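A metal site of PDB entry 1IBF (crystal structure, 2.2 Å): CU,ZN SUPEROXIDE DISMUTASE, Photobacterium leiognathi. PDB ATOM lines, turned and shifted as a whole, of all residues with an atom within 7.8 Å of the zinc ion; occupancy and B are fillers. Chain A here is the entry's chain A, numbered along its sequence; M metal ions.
The backbone NH of His 79 sits at hydrogen-bond distance from the side-chain carboxylate of Asp 133 (3.0 Å).
The backbone NH (N) of Gly 80 sits at hydrogen-bond distance from the side-chain carboxylate (OD2) of Asp 91, at 3.0 Å.
The backbone carbonyl oxygen of His 88 lies within hydrogen-bond range of the guanidinium group of Arg 111, at 2.8 Å.
The side-chain carboxylate (OD2) of Asp 91 lies within hydrogen-bond range of the side-chain amide nitrogen (ND2) of Asn 87.
NE2 of His 79 lies within hydrogen-bond range of OD1 of Asp 129, at 2.8 Å.
O of Lys 78 is in hydrogen-bond range of N of His 88 (2.8 Å).
The backbone NH (N) of His 88 sits at hydrogen-bond distance from the side-chain hydroxyl (OG1) of Thr 76.
A ring nitrogen (NE2) of His 70 lies close to a ring nitrogen (ND1) of His 45.
Of the 27 residues printed, 4 come within 4 Å of the zinc ion.
The nearest printed residue that does not touch the zinc ion is Lys 78 (4.6 Å).
The zinc ion is bound by OD1 of Asp 91 (1.9 Å).
A ring nitrogen (ND1) of His 70 is bound to the zinc ion.
The zinc ion is bound by ND1 of His 79 (2.1 Å).
A ring nitrogen (ND1) of His 88 binds the zinc ion (2.2 Å).
The zinc ion has four donor atoms within binding distance.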
ATOM      1  N   PHE A  44      11.291 -11.441  23.142  1.00  0.00           N
ATOM      2  CA  PHE A  44      10.149 -12.116  22.532  1.00  0.00           C
ATOM      3  C   PHE A  44       8.989 -11.136  22.369  1.00  0.00           C
ATOM      4  O   PHE A  44       8.381 -10.739  23.361  1.00  0.00           O
ATOM      5  CB  PHE A  44       9.694 -13.235  23.428  1.00  0.00           C
ATOM      6  CG  PHE A  44       8.751 -14.245  22.846  1.00  0.00           C
ATOM      7  CD1 PHE A  44       8.870 -14.703  21.544  1.00  0.00           C
ATOM      8  CD2 PHE A  44       7.774 -14.768  23.675  1.00  0.00           C
ATOM      9  CE1 PHE A  44       8.027 -15.698  21.065  1.00  0.00           C
ATOM     10  CE2 PHE A  44       6.921 -15.760  23.197  1.00  0.00           C
ATOM     11  CZ  PHE A  44       7.054 -16.212  21.899  1.00  0.00           C
ATOM     12  N   HIS A  45       8.653 -10.736  21.136  1.00  0.00           N
ATOM     13  CA  HIS A  45       7.578  -9.774  20.915  1.00  0.00           C
ATOM     14  C   HIS A  45       6.763 -10.051  19.675  1.00  0.00           C
ATOM     15  O   HIS A  45       7.206 -10.742  18.767  1.00  0.00           O
ATOM     16  CB  HIS A  45       8.121  -8.348  20.795  1.00  0.00           C
ATOM     17  CG  HIS A  45       9.469  -8.159  21.542  1.00  0.00           C
ATOM     18  ND1 HIS A  45      10.686  -8.046  20.908  1.00  0.00           N
ATOM     19  CD2 HIS A  45       9.722  -8.057  22.865  1.00  0.00           C
ATOM     20  CE1 HIS A  45      11.640  -7.887  21.808  1.00  0.00           C
ATOM     21  NE2 HIS A  45      11.084  -7.887  23.009  1.00  0.00           N
ATOM     22  N   ILE A  46       5.549  -9.513  19.658  1.00  0.00           N
ATOM     23  CA  ILE A  46       4.725  -9.655  18.468  1.00  0.00           C
ATOM     24  C   ILE A  46       5.098  -8.403  17.660  1.00  0.00           C
ATOM     25  O   ILE A  46       5.261  -7.329  18.241  1.00  0.00           O
ATOM     26  CB  ILE A  46       3.205  -9.578  18.756  1.00  0.00           C
ATOM     27  CG1 ILE A  46       2.740 -10.751  19.648  1.00  0.00           C
ATOM     28  CG2 ILE A  46       2.456  -9.540  17.423  1.00  0.00           C
ATOM     29  CD1 ILE A  46       3.059 -12.149  19.101  1.00  0.00           C
ATOM     30  N   HIS A  47       5.232  -8.532  16.355  1.00  0.00           N
ATOM     31  CA  HIS A  47       5.607  -7.382  15.510  1.00  0.00           C
ATOM     32  C   HIS A  47       4.476  -6.923  14.615  1.00  0.00           C
ATOM     33  O   HIS A  47       3.531  -7.671  14.351  1.00  0.00           O
ATOM     34  CB  HIS A  47       6.820  -7.707  14.633  1.00  0.00           C
ATOM     35  CG  HIS A  47       8.126  -7.398  15.365  1.00  0.00           C
ATOM     36  ND1 HIS A  47       8.987  -6.384  15.015  1.00  0.00           N
ATOM     37  CD2 HIS A  47       8.657  -7.990  16.460  1.00  0.00           C
ATOM     38  CE1 HIS A  47       9.995  -6.356  15.870  1.00  0.00           C
ATOM     39  NE2 HIS A  47       9.821  -7.326  16.758  1.00  0.00           N
ATOM     40  N   GLY A  69       8.321  -2.674  13.427  1.00  0.00           N
ATOM     41  CA  GLY A  69       8.558  -2.558  14.856  1.00  0.00           C
ATOM     42  C   GLY A  69       7.625  -3.421  15.687  1.00  0.00           C
ATOM     43  O   GLY A  69       6.870  -4.223  15.149  1.00  0.00           O
ATOM     44  N   HIS A  70       7.680  -3.247  17.006  1.00  0.00           N
ATOM     45  CA  HIS A  70       6.841  -3.998  17.940  1.00  0.00           C
ATOM     46  C   HIS A  70       5.371  -3.648  17.772  1.00  0.00           C
ATOM     47  O   HIS A  70       5.018  -2.496  17.520  1.00  0.00           O
ATOM     48  CB  HIS A  70       7.246  -3.695  19.401  1.00  0.00           C
ATOM     49  CG  HIS A  70       8.619  -4.154  19.776  1.00  0.00           C
ATOM     50  ND1 HIS A  70       9.104  -4.083  21.060  1.00  0.00           N
ATOM     51  CD2 HIS A  70       9.615  -4.694  19.036  1.00  0.00           C
ATOM     52  CE1 HIS A  70      10.337  -4.547  21.102  1.00  0.00           C
ATOM     53  NE2 HIS A  70      10.673  -4.933  19.883  1.00  0.00           N
ATOM     54  N   TYR A  71       4.506  -4.653  17.915  1.00  0.00           N
ATOM     55  CA  TYR A  71       3.070  -4.423  17.794  1.00  0.00           C
ATOM     56  C   TYR A  71       2.719  -3.347  18.831  1.00  0.00           C
ATOM     57  O   TYR A  71       3.027  -3.495  20.012  1.00  0.00           O
ATOM     58  CB  TYR A  71       2.330  -5.732  18.084  1.00  0.00           C
ATOM     59  CG  TYR A  71       0.815  -5.646  18.034  1.00  0.00           C
ATOM     60  CD1 TYR A  71       0.162  -4.992  16.991  1.00  0.00           C
ATOM     61  CD2 TYR A  71       0.049  -6.270  19.011  1.00  0.00           C
ATOM     62  CE1 TYR A  71      -1.230  -4.972  16.921  1.00  0.00           C
ATOM     63  CE2 TYR A  71      -1.334  -6.257  18.949  1.00  0.00           C
ATOM     64  CZ  TYR A  71      -1.974  -5.599  17.908  1.00  0.00           C
ATOM     65  OH  TYR A  71      -3.353  -5.611  17.869  1.00  0.00           O
ATOM     66  N   ASP A  72       2.093  -2.270  18.358  1.00  0.00           N
ATOM     67  CA  ASP A  72       1.741  -1.148  19.206  1.00  0.00           C
ATOM     68  C   ASP A  72       0.462  -0.466  18.710  1.00  0.00           C
ATOM     69  O   ASP A  72       0.494   0.678  18.243  1.00  0.00           O
ATOM     70  CB  ASP A  72       2.904  -0.152  19.193  1.00  0.00           C
ATOM     71  CG  ASP A  72       2.706   1.008  20.149  1.00  0.00           C
ATOM     72  OD1 ASP A  72       1.979   0.858  21.146  1.00  0.00           O
ATOM     73  OD2 ASP A  72       3.295   2.074  19.901  1.00  0.00           O
ATOM     74  N   THR A  76       1.933   3.808  21.620  1.00  0.00           N
ATOM     75  CA  THR A  76       2.589   4.304  22.815  1.00  0.00           C
ATOM     76  C   THR A  76       4.025   4.721  22.515  1.00  0.00           C
ATOM     77  O   THR A  76       4.589   5.583  23.186  1.00  0.00           O
ATOM     78  CB  THR A  76       2.645   3.218  23.889  1.00  0.00           C
ATOM     79  OG1 THR A  76       3.463   2.139  23.406  1.00  0.00           O
ATOM     80  CG2 THR A  76       1.249   2.706  24.181  1.00  0.00           C
ATOM     81  N   ASN A  77       4.614   4.073  21.516  1.00  0.00           N
ATOM     82  CA  ASN A  77       5.994   4.359  21.141  1.00  0.00           C
ATOM     83  C   ASN A  77       6.969   4.164  22.310  1.00  0.00           C
ATOM     84  O   ASN A  77       7.965   4.883  22.422  1.00  0.00           O
ATOM     85  N   LYS A  78       6.669   3.207  23.183  1.00  0.00           N
ATOM     86  CA  LYS A  78       7.515   2.905  24.314  1.00  0.00           C
ATOM     87  C   LYS A  78       7.561   1.386  24.462  1.00  0.00           C
ATOM     88  O   LYS A  78       6.638   0.676  24.051  1.00  0.00           O
ATOM     89  CB  LYS A  78       6.953   3.530  25.602  1.00  0.00           C
ATOM     90  CG  LYS A  78       6.846   5.053  25.595  1.00  0.00           C
ATOM     91  CD  LYS A  78       6.360   5.577  26.953  1.00  0.00           C
ATOM     92  CE  LYS A  78       6.291   7.098  27.015  1.00  0.00           C
ATOM     93  NZ  LYS A  78       5.122   7.673  26.279  1.00  0.00           N
ATOM     94  N   HIS A  79       8.644   0.875  25.043  1.00  0.00           N
ATOM     95  CA  HIS A  79       8.805  -0.551  25.242  1.00  0.00           C
ATOM     96  C   HIS A  79       8.746  -0.814  26.749  1.00  0.00           C
ATOM     97  O   HIS A  79       9.419  -0.145  27.528  1.00  0.00           O
ATOM     98  CB  HIS A  79      10.135  -1.004  24.646  1.00  0.00           C
ATOM     99  CG  HIS A  79      10.427  -2.453  24.856  1.00  0.00           C
ATOM    100  ND1 HIS A  79       9.787  -3.452  24.138  1.00  0.00           N
ATOM    101  CD2 HIS A  79      11.227  -3.081  25.747  1.00  0.00           C
ATOM    102  CE1 HIS A  79      10.189  -4.633  24.579  1.00  0.00           C
ATOM    103  NE2 HIS A  79      11.069  -4.433  25.557  1.00  0.00           N
ATOM    104  N   GLY A  80       7.919  -1.784  27.175  1.00  0.00           N
ATOM    105  CA  GLY A  80       7.806  -2.059  28.606  1.00  0.00           C
ATOM    106  C   GLY A  80       7.440  -3.478  28.997  1.00  0.00           C
ATOM    107  O   GLY A  80       7.850  -4.429  28.331  1.00  0.00           O
ATOM    108  N   PHE A  81       6.685  -3.639  30.087  1.00  0.00           N
ATOM    109  CA  PHE A  81       6.306  -4.969  30.551  1.00  0.00           C
ATOM    110  C   PHE A  81       5.046  -5.512  29.870  1.00  0.00           C
ATOM    111  O   PHE A  81       4.322  -4.790  29.183  1.00  0.00           O
ATOM    112  CB  PHE A  81       6.120  -4.974  32.077  1.00  0.00           C
ATOM    113  CG  PHE A  81       7.360  -4.620  32.846  1.00  0.00           C
ATOM    114  CD1 PHE A  81       7.694  -3.293  33.082  1.00  0.00           C
ATOM    115  CD2 PHE A  81       8.228  -5.615  33.288  1.00  0.00           C
ATOM    116  CE1 PHE A  81       8.868  -2.952  33.763  1.00  0.00           C
ATOM    117  CE2 PHE A  81       9.417  -5.289  33.963  1.00  0.00           C
ATOM    118  CZ  PHE A  81       9.733  -3.951  34.192  1.00  0.00           C
ATOM    119  N   ASN A  87       2.918   0.943  26.839  1.00  0.00           N
ATOM    120  CA  ASN A  87       4.044   0.472  26.065  1.00  0.00           C
ATOM    121  C   ASN A  87       3.495  -0.528  25.056  1.00  0.00           C
ATOM    122  O   ASN A  87       2.338  -0.959  25.173  1.00  0.00           O
ATOM    123  CB  ASN A  87       5.146  -0.144  26.941  1.00  0.00           C
ATOM    124  CG  ASN A  87       4.669  -1.309  27.781  1.00  0.00           C
ATOM    125  OD1 ASN A  87       4.243  -1.121  28.924  1.00  0.00           O
ATOM    126  ND2 ASN A  87       4.737  -2.515  27.224  1.00  0.00           N
ATOM    127  N   HIS A  88       4.299  -0.859  24.054  1.00  0.00           N
ATOM    128  CA  HIS A  88       3.889  -1.789  23.001  1.00  0.00           C
ATOM    129  C   HIS A  88       3.041  -2.958  23.533  1.00  0.00           C
ATOM    130  O   HIS A  88       3.471  -3.708  24.405  1.00  0.00           O
ATOM    131  CB  HIS A  88       5.136  -2.354  22.292  1.00  0.00           C
ATOM    132  CG  HIS A  88       6.106  -1.308  21.834  1.00  0.00           C
ATOM    133  ND1 HIS A  88       7.468  -1.490  21.893  1.00  0.00           N
ATOM    134  CD2 HIS A  88       5.918  -0.076  21.301  1.00  0.00           C
ATOM    135  CE1 HIS A  88       8.079  -0.423  21.405  1.00  0.00           C
ATOM    136  NE2 HIS A  88       7.162   0.451  21.036  1.00  0.00           N
ATOM    137  N   LYS A  89       1.837  -3.097  22.998  1.00  0.00           N
ATOM    138  CA  LYS A  89       0.934  -4.150  23.392  1.00  0.00           C
ATOM    139  C   LYS A  89       1.521  -5.515  22.958  1.00  0.00           C
ATOM    140  O   LYS A  89       1.071  -6.571  23.409  1.00  0.00           O
ATOM    141  CB  LYS A  89      -0.429  -3.911  22.730  1.00  0.00           C
ATOM    142  CG  LYS A  89      -1.588  -4.731  23.253  1.00  0.00           C
ATOM    143  N   GLY A  90       2.524  -5.461  22.094  1.00  0.00           N
ATOM    144  CA  GLY A  90       3.150  -6.676  21.589  1.00  0.00           C
ATOM    145  C   GLY A  90       4.304  -7.203  22.433  1.00  0.00           C
ATOM    146  O   GLY A  90       4.913  -8.214  22.086  1.00  0.00           O
ATOM    147  N   ASP A  91       4.588  -6.502  23.526  1.00  0.00           N
ATOM    148  CA  ASP A  91       5.665  -6.903  24.422  1.00  0.00           C
ATOM    149  C   ASP A  91       5.270  -8.157  25.228  1.00  0.00           C
ATOM    150  O   ASP A  91       4.313  -8.155  26.012  1.00  0.00           O
ATOM    151  CB  ASP A  91       6.012  -5.744  25.377  1.00  0.00           C
ATOM    152  CG  ASP A  91       6.588  -4.540  24.639  1.00  0.00           C
ATOM    153  OD1 ASP A  91       7.158  -4.727  23.542  1.00  0.00           O
ATOM    154  OD2 ASP A  91       6.485  -3.418  25.155  1.00  0.00           O
ATOM    155  N   LEU A  92       6.031  -9.224  25.011  1.00  0.00           N
ATOM    156  CA  LEU A  92       5.800 -10.516  25.658  1.00  0.00           C
ATOM    157  C   LEU A  92       6.904 -10.789  26.681  1.00  0.00           C
ATOM    158  O   LEU A  92       7.922 -10.101  26.692  1.00  0.00           O
ATOM    159  CB  LEU A  92       5.805 -11.624  24.590  1.00  0.00           C
ATOM    160  CG  LEU A  92       4.910 -11.480  23.338  1.00  0.00           C
ATOM    161  CD1 LEU A  92       5.243 -12.583  22.320  1.00  0.00           C
ATOM    162  CD2 LEU A  92       3.453 -11.551  23.750  1.00  0.00           C
ATOM    163  N   ARG A 111      -2.430  -8.853  28.125  1.00  0.00           N
ATOM    164  CA  ARG A 111      -3.045  -7.743  27.404  1.00  0.00           C
ATOM    165  C   ARG A 111      -3.469  -8.076  25.971  1.00  0.00           C
ATOM    166  O   ARG A 111      -4.099  -7.249  25.306  1.00  0.00           O
ATOM    167  CB  ARG A 111      -2.106  -6.540  27.379  1.00  0.00           C
ATOM    168  CG  ARG A 111      -1.939  -5.811  28.707  1.00  0.00           C
ATOM    169  CD  ARG A 111      -1.250  -4.477  28.457  1.00  0.00           C
ATOM    170  NE  ARG A 111       0.109  -4.662  28.019  1.00  0.00           N
ATOM    171  CZ  ARG A 111       0.724  -3.938  27.088  1.00  0.00           C
ATOM    172  NH1 ARG A 111       0.100  -2.935  26.471  1.00  0.00           N
ATOM    173  NH2 ARG A 111       1.991  -4.223  26.762  1.00  0.00           N
ATOM    174  N   ASP A 129      15.594  -9.054  27.271  1.00  0.00           N
ATOM    175  CA  ASP A 129      14.568  -8.024  27.306  1.00  0.00           C
ATOM    176  C   ASP A 129      14.366  -7.560  28.737  1.00  0.00           C
ATOM    177  O   ASP A 129      13.765  -8.275  29.541  1.00  0.00           O
ATOM    178  CB  ASP A 129      13.245  -8.597  26.762  1.00  0.00           C
ATOM    179  CG  ASP A 129      12.188  -7.532  26.557  1.00  0.00           C
ATOM    180  OD1 ASP A 129      12.321  -6.419  27.109  1.00  0.00           O
ATOM    181  OD2 ASP A 129      11.200  -7.829  25.845  1.00  0.00           O
ATOM    182  N   HIS A 131      12.648  -5.050  29.470  1.00  0.00           N
ATOM    183  CA  HIS A 131      11.403  -4.292  29.397  1.00  0.00           C
ATOM    184  C   HIS A 131      11.531  -2.791  29.597  1.00  0.00           C
ATOM    185  O   HIS A 131      10.753  -2.184  30.330  1.00  0.00           O
ATOM    186  CB  HIS A 131      10.389  -4.862  30.377  1.00  0.00           C
ATOM    187  CG  HIS A 131      10.087  -6.301  30.125  1.00  0.00           C
ATOM    188  ND1 HIS A 131      10.620  -7.323  30.881  1.00  0.00           N
ATOM    189  CD2 HIS A 131       9.379  -6.899  29.133  1.00  0.00           C
ATOM    190  CE1 HIS A 131      10.257  -8.488  30.363  1.00  0.00           C
ATOM    191  NE2 HIS A 131       9.511  -8.249  29.299  1.00  0.00           N
ATOM    192  N   SER A 132      12.511  -2.211  28.916  1.00  0.00           N
ATOM    193  CA  SER A 132      12.799  -0.793  28.981  1.00  0.00           C
ATOM    194  C   SER A 132      13.558  -0.407  27.720  1.00  0.00           C
ATOM    195  O   SER A 132      14.096  -1.267  27.028  1.00  0.00           O
ATOM    196  CB  SER A 132      13.669  -0.476  30.189  1.00  0.00           C
ATOM    197  OG  SER A 132      14.058   0.879  30.200  1.00  0.00           O
ATOM    198  N   ASP A 133      13.607   0.889  27.412  1.00  0.00           N
ATOM    199  CA  ASP A 133      14.348   1.372  26.259  1.00  0.00           C
ATOM    200  C   ASP A 133      15.720   1.866  26.728  1.00  0.00           C
ATOM    201  O   ASP A 133      16.437   2.555  25.999  1.00  0.00           O
ATOM    202  CB  ASP A 133      13.588   2.518  25.564  1.00  0.00           C
ATOM    203  CG  ASP A 133      12.464   2.012  24.691  1.00  0.00           C
ATOM    204  OD1 ASP A 133      12.745   1.278  23.717  1.00  0.00           O
ATOM    205  OD2 ASP A 133      11.285   2.344  24.968  1.00  0.00           O
ATOM    206  N   LEU A 138      14.324  -0.909  22.954  1.00  0.00           N
ATOM    207  CA  LEU A 138      13.563  -2.129  22.765  1.00  0.00           C
ATOM    208  C   LEU A 138      13.939  -3.275  23.716  1.00  0.00           C
ATOM    209  O   LEU A 138      13.662  -4.434  23.428  1.00  0.00           O
ATOM    210  CB  LEU A 138      13.720  -2.563  21.312  1.00  0.00           C
ATOM    211  CG  LEU A 138      13.515  -1.389  20.354  1.00  0.00           C
ATOM    212  CD1 LEU A 138      13.712  -1.838  18.919  1.00  0.00           C
ATOM    213  CD2 LEU A 138      12.101  -0.835  20.549  1.00  0.00           C
ATOM    214  N   GLY A 139      14.564  -2.933  24.838  1.00  0.00           N
ATOM    215  CA  GLY A 139      14.927  -3.945  25.816  1.00  0.00           C
ATOM    216  C   GLY A 139      16.241  -4.669  25.568  1.00  0.00           C
ATOM    217  O   GLY A 139      16.565  -5.635  26.267  1.00  0.00           O
HETATM  218 ZN    ZN M   1       8.205  -3.398  22.756  1.00  0.00          ZN
HETATM  219 CU    CU M   2      10.895  -8.018  18.711  1.00  0.00          CU
